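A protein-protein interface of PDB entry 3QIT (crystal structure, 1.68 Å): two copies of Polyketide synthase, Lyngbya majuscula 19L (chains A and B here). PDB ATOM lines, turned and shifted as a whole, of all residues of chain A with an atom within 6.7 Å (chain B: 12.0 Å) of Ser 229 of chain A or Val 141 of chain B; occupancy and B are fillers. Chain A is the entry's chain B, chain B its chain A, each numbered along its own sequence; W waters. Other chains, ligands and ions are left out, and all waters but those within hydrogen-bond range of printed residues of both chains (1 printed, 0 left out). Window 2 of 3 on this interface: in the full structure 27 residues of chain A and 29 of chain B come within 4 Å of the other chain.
Of chain B, only Val 141 (3.9 Å) comes within 4 Å of Ser 229 of chain A. Printed residues of chain A within 4 Å of Val 141 of chain B: Ser 114 and Ser 229. Of chain B, only Leu 144 (3.9 Å), Thr 145 (3.8 Å) and Leu 148 (3.8 Å) come within 4 Å of Val 115 of chain A. Met 226 of chain A touches one residue of chain B. No residue of chain B comes within 4 Å of Lys 228 of chain A. No residue of chain B comes within 4 Å of Gln 231 of chain A. Of the printed residues of chain A, Leu 148 of chain B touches Val 115. Printed residues of chain A within 4 Å of Thr 145 of chain B: Val 115. Printed residues of chain A within 4 Å of Leu 144 of chain B: Val 115 (3.9 Å) and Met 226 (3.8 Å). The nearest residue of chain B that does not touch Ser 229 of chain A is Ser 139 of chain B (6.5 Å). The nearest printed residue of chain A that does not touch Leu 148 of chain B is Ala 111 of chain A (6.0 Å).
Among the printed residues, pairs that only touch across the chains: Ser 114 of chain A with Val 141 of chain B, Val 115 of chain A with Leu 144 of chain B, Val 115 of chain A with Thr 145 of chain B, Val 115 of chain A with Leu 148 of chain B, Gln 222 of chain A with Ala 140 of chain B, Met 226 of chain A with Leu 144 of chain B and Ser 229 of chain A with Val 141 of chain B.
The backbone carbonyl oxygen of Val 141 of chain B is in hydrogen-bond range of the side-chain hydroxyl of Thr 145 of chain B (3.0 Å). OG of Ser 114 of chain A is in hydrogen-bond range of O of Ala 111 of chain A (2.7 Å). O of Met 226 of chain A lies within hydrogen-bond range of OG of Ser 229 of chain A.
Printed residues of chain B that touch a printed residue of chain A: Ala 140, Val 141, Leu 144, Thr 145 and Leu 148. Hydrophobic or aromatic side chains of chain B within 4 Å of the printed part of chain A: Ala 140, Val 141, Leu 144 and Leu 148. Hydrophobic or aromatic side chains of chain A within 4 Å of the printed part of chain B: Val 115 and Met 226. Among the printed residues, 7 pairs touch across the chains. Among the printed residues, no Asp or Glu carboxylate lies within 4 Å of a Lys or Arg side-chain nitrogen of the other chain.
Water W1 lies within hydrogen-bond range of the side-chain hydroxyl of Thr 145 of chain B, the backbone carbonyl oxygen of Val 115 of chain A and the backbone carbonyl oxygen of Ser 114 of chain A.
No position is printed for both chains.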
ATOM      1  N   ALA A 111      -5.612 -17.032   7.439  1.00  0.00           N
ATOM      2  CA  ALA A 111      -6.687 -16.420   8.187  1.00  0.00           C
ATOM      3  C   ALA A 111      -7.121 -17.315   9.332  1.00  0.00           C
ATOM      4  O   ALA A 111      -7.254 -16.858  10.477  1.00  0.00           O
ATOM      5  CB  ALA A 111      -7.844 -16.064   7.269  1.00  0.00           C
ATOM      6  N   SER A 114      -4.609 -17.292  12.075  1.00  0.00           N
ATOM      7  CA  SER A 114      -4.643 -16.024  12.816  1.00  0.00           C
ATOM      8  C   SER A 114      -5.741 -16.031  13.871  1.00  0.00           C
ATOM      9  O   SER A 114      -5.575 -15.451  14.948  1.00  0.00           O
ATOM     10  CB  SER A 114      -4.761 -14.816  11.868  1.00  0.00           C
ATOM     11  OG  SER A 114      -6.085 -14.616  11.391  1.00  0.00           O
ATOM     12  N   VAL A 115      -6.834 -16.728  13.567  1.00  0.00           N
ATOM     13  CA  VAL A 115      -8.006 -16.834  14.441  1.00  0.00           C
ATOM     14  C   VAL A 115      -7.893 -17.949  15.489  1.00  0.00           C
ATOM     15  O   VAL A 115      -8.312 -17.766  16.636  1.00  0.00           O
ATOM     16  CB  VAL A 115      -9.302 -17.014  13.604  1.00  0.00           C
ATOM     17  CG1 VAL A 115     -10.521 -17.335  14.488  1.00  0.00           C
ATOM     18  CG2 VAL A 115      -9.567 -15.769  12.767  1.00  0.00           C
ATOM     19  N   GLN A 222      -3.994  -4.151   4.901  1.00  0.00           N
ATOM     20  CA  GLN A 222      -4.670  -4.888   5.969  1.00  0.00           C
ATOM     21  C   GLN A 222      -4.198  -6.347   6.033  1.00  0.00           C
ATOM     22  O   GLN A 222      -3.974  -6.891   7.125  1.00  0.00           O
ATOM     23  CB  GLN A 222      -6.189  -4.828   5.777  1.00  0.00           C
ATOM     24  CG  GLN A 222      -7.005  -5.315   6.968  1.00  0.00           C
ATOM     25  CD  GLN A 222      -7.331  -4.206   7.967  1.00  0.00           C
ATOM     26  OE1 GLN A 222      -6.435  -3.562   8.523  1.00  0.00           O
ATOM     27  NE2 GLN A 222      -8.623  -3.991   8.208  1.00  0.00           N
ATOM     28  N   LEU A 224      -1.312  -7.639   5.080  1.00  0.00           N
ATOM     29  CA  LEU A 224       0.030  -7.713   5.654  1.00  0.00           C
ATOM     30  C   LEU A 224      -0.031  -7.626   7.177  1.00  0.00           C
ATOM     31  O   LEU A 224       0.749  -8.283   7.873  1.00  0.00           O
ATOM     32  CB  LEU A 224       0.935  -6.610   5.094  1.00  0.00           C
ATOM     33  CG  LEU A 224       1.296  -6.686   3.603  1.00  0.00           C
ATOM     34  CD1 LEU A 224       2.139  -5.478   3.195  1.00  0.00           C
ATOM     35  CD2 LEU A 224       2.026  -7.989   3.281  1.00  0.00           C
ATOM     36  N   GLU A 225      -0.964  -6.835   7.701  1.00  0.00           N
ATOM     37  CA  GLU A 225      -1.106  -6.756   9.148  1.00  0.00           C
ATOM     38  C   GLU A 225      -1.535  -8.104   9.722  1.00  0.00           C
ATOM     39  O   GLU A 225      -1.078  -8.490  10.798  1.00  0.00           O
ATOM     40  CB  GLU A 225      -2.060  -5.633   9.573  1.00  0.00           C
ATOM     41  CG  GLU A 225      -1.496  -4.222   9.369  1.00  0.00           C
ATOM     42  CD  GLU A 225      -0.337  -3.874  10.312  1.00  0.00           C
ATOM     43  OE1 GLU A 225       0.372  -2.876  10.035  1.00  0.00           O
ATOM     44  OE2 GLU A 225      -0.132  -4.578  11.330  1.00  0.00           O
ATOM     45  N   MET A 226      -2.398  -8.814   8.998  1.00  0.00           N
ATOM     46  CA  MET A 226      -2.779 -10.175   9.375  1.00  0.00           C
ATOM     47  C   MET A 226      -1.540 -11.068   9.405  1.00  0.00           C
ATOM     48  O   MET A 226      -1.292 -11.754  10.407  1.00  0.00           O
ATOM     49  CB  MET A 226      -3.834 -10.738   8.411  1.00  0.00           C
ATOM     50  CG  MET A 226      -3.907 -12.272   8.358  1.00  0.00           C
ATOM     51  SD  MET A 226      -5.368 -12.897   7.514  1.00  0.00           S
ATOM     52  CE  MET A 226      -6.597 -12.586   8.773  1.00  0.00           C
ATOM     53  N   LEU A 227      -0.768 -11.040   8.315  1.00  0.00           N
ATOM     54  CA  LEU A 227       0.447 -11.860   8.196  1.00  0.00           C
ATOM     55  C   LEU A 227       1.444 -11.553   9.321  1.00  0.00           C
ATOM     56  O   LEU A 227       2.038 -12.470   9.912  1.00  0.00           O
ATOM     57  CB  LEU A 227       1.116 -11.673   6.830  1.00  0.00           C
ATOM     58  CG  LEU A 227       0.365 -12.090   5.548  1.00  0.00           C
ATOM     59  CD1 LEU A 227       1.229 -11.893   4.333  1.00  0.00           C
ATOM     60  CD2 LEU A 227      -0.155 -13.520   5.603  1.00  0.00           C
ATOM     61  N   LYS A 228       1.575 -10.269   9.643  1.00  0.00           N
ATOM     62  CA  LYS A 228       2.484  -9.825  10.695  1.00  0.00           C
ATOM     63  C   LYS A 228       2.096 -10.409  12.058  1.00  0.00           C
ATOM     64  O   LYS A 228       2.971 -10.686  12.880  1.00  0.00           O
ATOM     65  CB  LYS A 228       2.525  -8.290  10.745  1.00  0.00           C
ATOM     66  CG  LYS A 228       3.731  -7.717  11.469  1.00  0.00           C
ATOM     67  CD  LYS A 228       3.713  -6.190  11.492  1.00  0.00           C
ATOM     68  CE  LYS A 228       4.959  -5.641  12.194  1.00  0.00           C
ATOM     69  NZ  LYS A 228       4.877  -4.172  12.475  1.00  0.00           N
ATOM     70  N   SER A 229       0.792 -10.615  12.263  1.00  0.00           N
ATOM     71  CA  SER A 229       0.221 -11.041  13.552  1.00  0.00           C
ATOM     72  C   SER A 229       0.344 -12.542  13.841  1.00  0.00           C
ATOM     73  O   SER A 229       0.185 -12.975  14.999  1.00  0.00           O
ATOM     74  CB  SER A 229      -1.258 -10.641  13.631  1.00  0.00           C
ATOM     75  OG  SER A 229      -2.092 -11.554  12.921  1.00  0.00           O
ATOM     76  N   ILE A 230       0.617 -13.325  12.799  1.00  0.00           N
ATOM     77  CA  ILE A 230       0.685 -14.787  12.874  1.00  0.00           C
ATOM     78  C   ILE A 230       1.721 -15.193  13.940  1.00  0.00           C
ATOM     79  O   ILE A 230       2.900 -14.878  13.775  1.00  0.00           O
ATOM     80  CB  ILE A 230       1.060 -15.410  11.475  1.00  0.00           C
ATOM     81  CG1 ILE A 230       0.037 -15.045  10.374  1.00  0.00           C
ATOM     82  CG2 ILE A 230       1.224 -16.928  11.583  1.00  0.00           C
ATOM     83  CD1 ILE A 230       0.544 -15.227   8.873  1.00  0.00           C
ATOM     84  N   GLN A 231       1.290 -15.883  14.993  1.00  0.00           N
ATOM     85  CA  GLN A 231       2.199 -16.300  16.075  1.00  0.00           C
ATOM     86  C   GLN A 231       2.673 -17.747  15.953  1.00  0.00           C
ATOM     87  O   GLN A 231       3.664 -18.149  16.590  1.00  0.00           O
ATOM     88  CB  GLN A 231       1.542 -16.071  17.440  1.00  0.00           C
ATOM     89  CG  GLN A 231       1.450 -14.599  17.870  1.00  0.00           C
ATOM     90  CD  GLN A 231       2.765 -14.036  18.408  1.00  0.00           C
ATOM     91  OE1 GLN A 231       3.773 -13.974  17.698  1.00  0.00           O
ATOM     92  NE2 GLN A 231       2.749 -13.601  19.667  1.00  0.00           N
ATOM     93  N   VAL A 232       1.972 -18.505  15.112  1.00  0.00           N
ATOM     94  CA  VAL A 232       2.293 -19.914  14.946  1.00  0.00           C
ATOM     95  C   VAL A 232       3.519 -20.114  14.062  1.00  0.00           C
ATOM     96  O   VAL A 232       3.824 -19.298  13.189  1.00  0.00           O
ATOM     97  CB  VAL A 232       1.107 -20.767  14.409  1.00  0.00           C
ATOM     98  CG1 VAL A 232      -0.091 -20.693  15.354  1.00  0.00           C
ATOM     99  CG2 VAL A 232       0.740 -20.369  12.988  1.00  0.00           C
ATOM    100  N   THR A 256       7.469  -8.958   6.290  1.00  0.00           N
ATOM    101  CA  THR A 256       6.297  -8.980   7.138  1.00  0.00           C
ATOM    102  C   THR A 256       6.311 -10.129   8.133  1.00  0.00           C
ATOM    103  O   THR A 256       5.992  -9.935   9.306  1.00  0.00           O
ATOM    104  CB  THR A 256       5.039  -9.000   6.263  1.00  0.00           C
ATOM    105  OG1 THR A 256       5.041  -7.802   5.473  1.00  0.00           O
ATOM    106  CG2 THR A 256       3.787  -9.050   7.110  1.00  0.00           C
ATOM    107  N   GLU B 138      -9.706  -1.372  15.535  1.00  0.00           N
ATOM    108  CA  GLU B 138      -8.714  -2.396  15.878  1.00  0.00           C
ATOM    109  C   GLU B 138      -8.442  -3.366  14.720  1.00  0.00           C
ATOM    110  O   GLU B 138      -9.119  -3.316  13.690  1.00  0.00           O
ATOM    111  CB  GLU B 138      -9.114  -3.143  17.162  1.00  0.00           C
ATOM    112  CG  GLU B 138     -10.572  -3.606  17.220  1.00  0.00           C
ATOM    113  CD  GLU B 138     -11.157  -3.537  18.624  1.00  0.00           C
ATOM    114  OE1 GLU B 138     -10.924  -2.524  19.324  1.00  0.00           O
ATOM    115  OE2 GLU B 138     -11.860  -4.491  19.020  1.00  0.00           O
ATOM    116  N   SER B 139      -7.454  -4.242  14.907  1.00  0.00           N
ATOM    117  CA  SER B 139      -6.974  -5.156  13.861  1.00  0.00           C
ATOM    118  C   SER B 139      -8.063  -6.002  13.206  1.00  0.00           C
ATOM    119  O   SER B 139      -9.068  -6.343  13.837  1.00  0.00           O
ATOM    120  CB  SER B 139      -5.904  -6.089  14.428  1.00  0.00           C
ATOM    121  OG  SER B 139      -6.499  -7.144  15.165  1.00  0.00           O
ATOM    122  N   ALA B 140      -7.835  -6.347  11.941  1.00  0.00           N
ATOM    123  CA  ALA B 140      -8.728  -7.223  11.189  1.00  0.00           C
ATOM    124  C   ALA B 140      -8.779  -8.635  11.771  1.00  0.00           C
ATOM    125  O   ALA B 140      -9.830  -9.269  11.744  1.00  0.00           O
ATOM    126  CB  ALA B 140      -8.319  -7.275   9.719  1.00  0.00           C
ATOM    127  N   VAL B 141      -7.644  -9.122  12.282  1.00  0.00           N
ATOM    128  CA  VAL B 141      -7.600 -10.448  12.912  1.00  0.00           C
ATOM    129  C   VAL B 141      -8.564 -10.527  14.093  1.00  0.00           C
ATOM    130  O   VAL B 141      -9.350 -11.472  14.192  1.00  0.00           O
ATOM    131  CB  VAL B 141      -6.152 -10.907  13.331  1.00  0.00           C
ATOM    132  CG1 VAL B 141      -5.393  -9.810  14.080  1.00  0.00           C
ATOM    133  CG2 VAL B 141      -6.202 -12.191  14.158  1.00  0.00           C
ATOM    134  N   ASN B 142      -8.515  -9.522  14.968  1.00  0.00           N
ATOM    135  CA  ASN B 142      -9.384  -9.523  16.133  1.00  0.00           C
ATOM    136  C   ASN B 142     -10.847  -9.345  15.735  1.00  0.00           C
ATOM    137  O   ASN B 142     -11.744  -9.904  16.382  1.00  0.00           O
ATOM    138  CB  ASN B 142      -8.909  -8.504  17.168  1.00  0.00           C
ATOM    139  CG  ASN B 142      -7.575  -8.904  17.799  1.00  0.00           C
ATOM    140  OD1 ASN B 142      -7.293 -10.096  17.990  1.00  0.00           O
ATOM    141  ND2 ASN B 142      -6.745  -7.916  18.110  1.00  0.00           N
ATOM    142  N   GLN B 143     -11.084  -8.596  14.658  1.00  0.00           N
ATOM    143  CA  GLN B 143     -12.408  -8.509  14.052  1.00  0.00           C
ATOM    144  C   GLN B 143     -12.885  -9.863  13.525  1.00  0.00           C
ATOM    145  O   GLN B 143     -14.054 -10.235  13.699  1.00  0.00           O
ATOM    146  CB  GLN B 143     -12.425  -7.460  12.929  1.00  0.00           C
ATOM    147  CG  GLN B 143     -13.185  -6.161  13.246  1.00  0.00           C
ATOM    148  CD  GLN B 143     -12.642  -5.397  14.455  1.00  0.00           C
ATOM    149  OE1 GLN B 143     -12.796  -5.827  15.603  1.00  0.00           O
ATOM    150  NE2 GLN B 143     -12.029  -4.244  14.197  1.00  0.00           N
ATOM    151  N   LEU B 144     -11.979 -10.595  12.878  1.00  0.00           N
ATOM    152  CA  LEU B 144     -12.311 -11.862  12.264  1.00  0.00           C
ATOM    153  C   LEU B 144     -12.600 -12.940  13.314  1.00  0.00           C
ATOM    154  O   LEU B 144     -13.494 -13.750  13.131  1.00  0.00           O
ATOM    155  CB  LEU B 144     -11.170 -12.303  11.365  1.00  0.00           C
ATOM    156  CG  LEU B 144     -11.467 -13.326  10.290  1.00  0.00           C
ATOM    157  CD1 LEU B 144     -12.487 -12.754   9.326  1.00  0.00           C
ATOM    158  CD2 LEU B 144     -10.158 -13.648   9.577  1.00  0.00           C
ATOM    159  N   THR B 145     -11.847 -12.918  14.418  1.00  0.00           N
ATOM    160  CA  THR B 145     -12.059 -13.845  15.549  1.00  0.00           C
ATOM    161  C   THR B 145     -13.449 -13.609  16.149  1.00  0.00           C
ATOM    162  O   THR B 145     -14.227 -14.551  16.295  1.00  0.00           O
ATOM    163  CB  THR B 145     -10.971 -13.676  16.635  1.00  0.00           C
ATOM    164  OG1 THR B 145      -9.677 -13.841  16.041  1.00  0.00           O
ATOM    165  CG2 THR B 145     -11.144 -14.675  17.792  1.00  0.00           C
ATOM    166  N   THR B 146     -13.759 -12.352  16.459  1.00  0.00           N
ATOM    167  CA  THR B 146     -15.088 -11.986  17.005  1.00  0.00           C
ATOM    168  C   THR B 146     -16.212 -12.454  16.086  1.00  0.00           C
ATOM    169  O   THR B 146     -17.237 -12.966  16.545  1.00  0.00           O
ATOM    170  CB  THR B 146     -15.168 -10.461  17.289  1.00  0.00           C
ATOM    171  OG1 THR B 146     -14.055 -10.102  18.117  1.00  0.00           O
ATOM    172  CG2 THR B 146     -16.479 -10.081  18.023  1.00  0.00           C
ATOM    173  N   CYS B 147     -15.994 -12.304  14.780  1.00  0.00           N
ATOM    174  CA  CYS B 147     -16.993 -12.629  13.786  1.00  0.00           C
ATOM    175  C   CYS B 147     -17.227 -14.144  13.722  1.00  0.00           C
ATOM    176  O   CYS B 147     -18.366 -14.594  13.795  1.00  0.00           O
ATOM    177  CB  CYS B 147     -16.598 -12.071  12.421  1.00  0.00           C
ATOM    178  SG  CYS B 147     -17.761 -12.500  11.110  1.00  0.00           S
ATOM    179  N   LEU B 148     -16.150 -14.922  13.632  1.00  0.00           N
ATOM    180  CA  LEU B 148     -16.260 -16.381  13.561  1.00  0.00           C
ATOM    181  C   LEU B 148     -16.863 -16.992  14.817  1.00  0.00           C
ATOM    182  O   LEU B 148     -17.654 -17.928  14.717  1.00  0.00           O
ATOM    183  CB  LEU B 148     -14.913 -17.033  13.250  1.00  0.00           C
ATOM    184  CG  LEU B 148     -14.381 -16.888  11.819  1.00  0.00           C
ATOM    185  CD1 LEU B 148     -13.114 -17.707  11.703  1.00  0.00           C
ATOM    186  CD2 LEU B 148     -15.385 -17.326  10.764  1.00  0.00           C
ATOM    187  N   ASP B 149     -16.501 -16.457  15.989  1.00  0.00           N
ATOM    188  CA  ASP B 149     -17.129 -16.902  17.247  1.00  0.00           C
ATOM    189  C   ASP B 149     -18.628 -16.562  17.245  1.00  0.00           C
ATOM    190  O   ASP B 149     -19.444 -17.376  17.677  1.00  0.00           O
ATOM    191  CB  ASP B 149     -16.474 -16.244  18.459  1.00  0.00           C
ATOM    192  CG  ASP B 149     -15.067 -16.743  18.696  1.00  0.00           C
ATOM    193  OD1 ASP B 149     -14.700 -17.804  18.122  1.00  0.00           O
ATOM    194  OD2 ASP B 149     -14.339 -16.077  19.458  1.00  0.00           O
ATOM    195  N   TYR B 150     -18.983 -15.384  16.750  1.00  0.00           N
ATOM    196  CA  TYR B 150     -20.400 -14.988  16.707  1.00  0.00           C
ATOM    197  C   TYR B 150     -21.208 -15.909  15.775  1.00  0.00           C
ATOM    198  O   TYR B 150     -22.310 -16.396  16.140  1.00  0.00           O
ATOM    199  CB  TYR B 150     -20.572 -13.503  16.324  1.00  0.00           C
ATOM    200  CG  TYR B 150     -22.025 -13.099  16.310  1.00  0.00           C
ATOM    201  CD1 TYR B 150     -22.792 -13.135  17.483  1.00  0.00           C
ATOM    202  CD2 TYR B 150     -22.660 -12.776  15.111  1.00  0.00           C
ATOM    203  CE1 TYR B 150     -24.167 -12.810  17.463  1.00  0.00           C
ATOM    204  CE2 TYR B 150     -24.030 -12.463  15.083  1.00  0.00           C
ATOM    205  CZ  TYR B 150     -24.760 -12.462  16.266  1.00  0.00           C
ATOM    206  OH  TYR B 150     -26.113 -12.157  16.234  1.00  0.00           O
ATOM    207  N   LEU B 151     -20.662 -16.157  14.583  1.00  0.00           N
ATOM    208  CA  LEU B 151     -21.343 -16.991  13.574  1.00  0.00           C
ATOM    209  C   LEU B 151     -21.704 -18.385  14.103  1.00  0.00           C
ATOM    210  O   LEU B 151     -22.689 -18.968  13.664  1.00  0.00           O
ATOM    211  CB  LEU B 151     -20.494 -17.163  12.305  1.00  0.00           C
ATOM    212  CG  LEU B 151     -19.943 -15.972  11.510  1.00  0.00           C
ATOM    213  CD1 LEU B 151     -18.926 -16.461  10.471  1.00  0.00           C
ATOM    214  CD2 LEU B 151     -21.013 -15.130  10.873  1.00  0.00           C
ATOM    215  N   ILE B 210     -21.710  -6.897  14.089  1.00  0.00           N
ATOM    216  CA  ILE B 210     -20.728  -7.965  13.897  1.00  0.00           C
ATOM    217  C   ILE B 210     -20.935  -8.715  12.566  1.00  0.00           C
ATOM    218  O   ILE B 210     -19.973  -9.118  11.910  1.00  0.00           O
ATOM    219  CB  ILE B 210     -20.684  -8.912  15.128  1.00  0.00           C
ATOM    220  CG1 ILE B 210     -20.240  -8.097  16.344  1.00  0.00           C
ATOM    221  CG2 ILE B 210     -19.696 -10.054  14.899  1.00  0.00           C
ATOM    222  CD1 ILE B 210     -20.221  -8.851  17.614  1.00  0.00           C
HETATM  223  O   HOH W   1      -7.578 -14.924  17.686  1.00  0.00           O
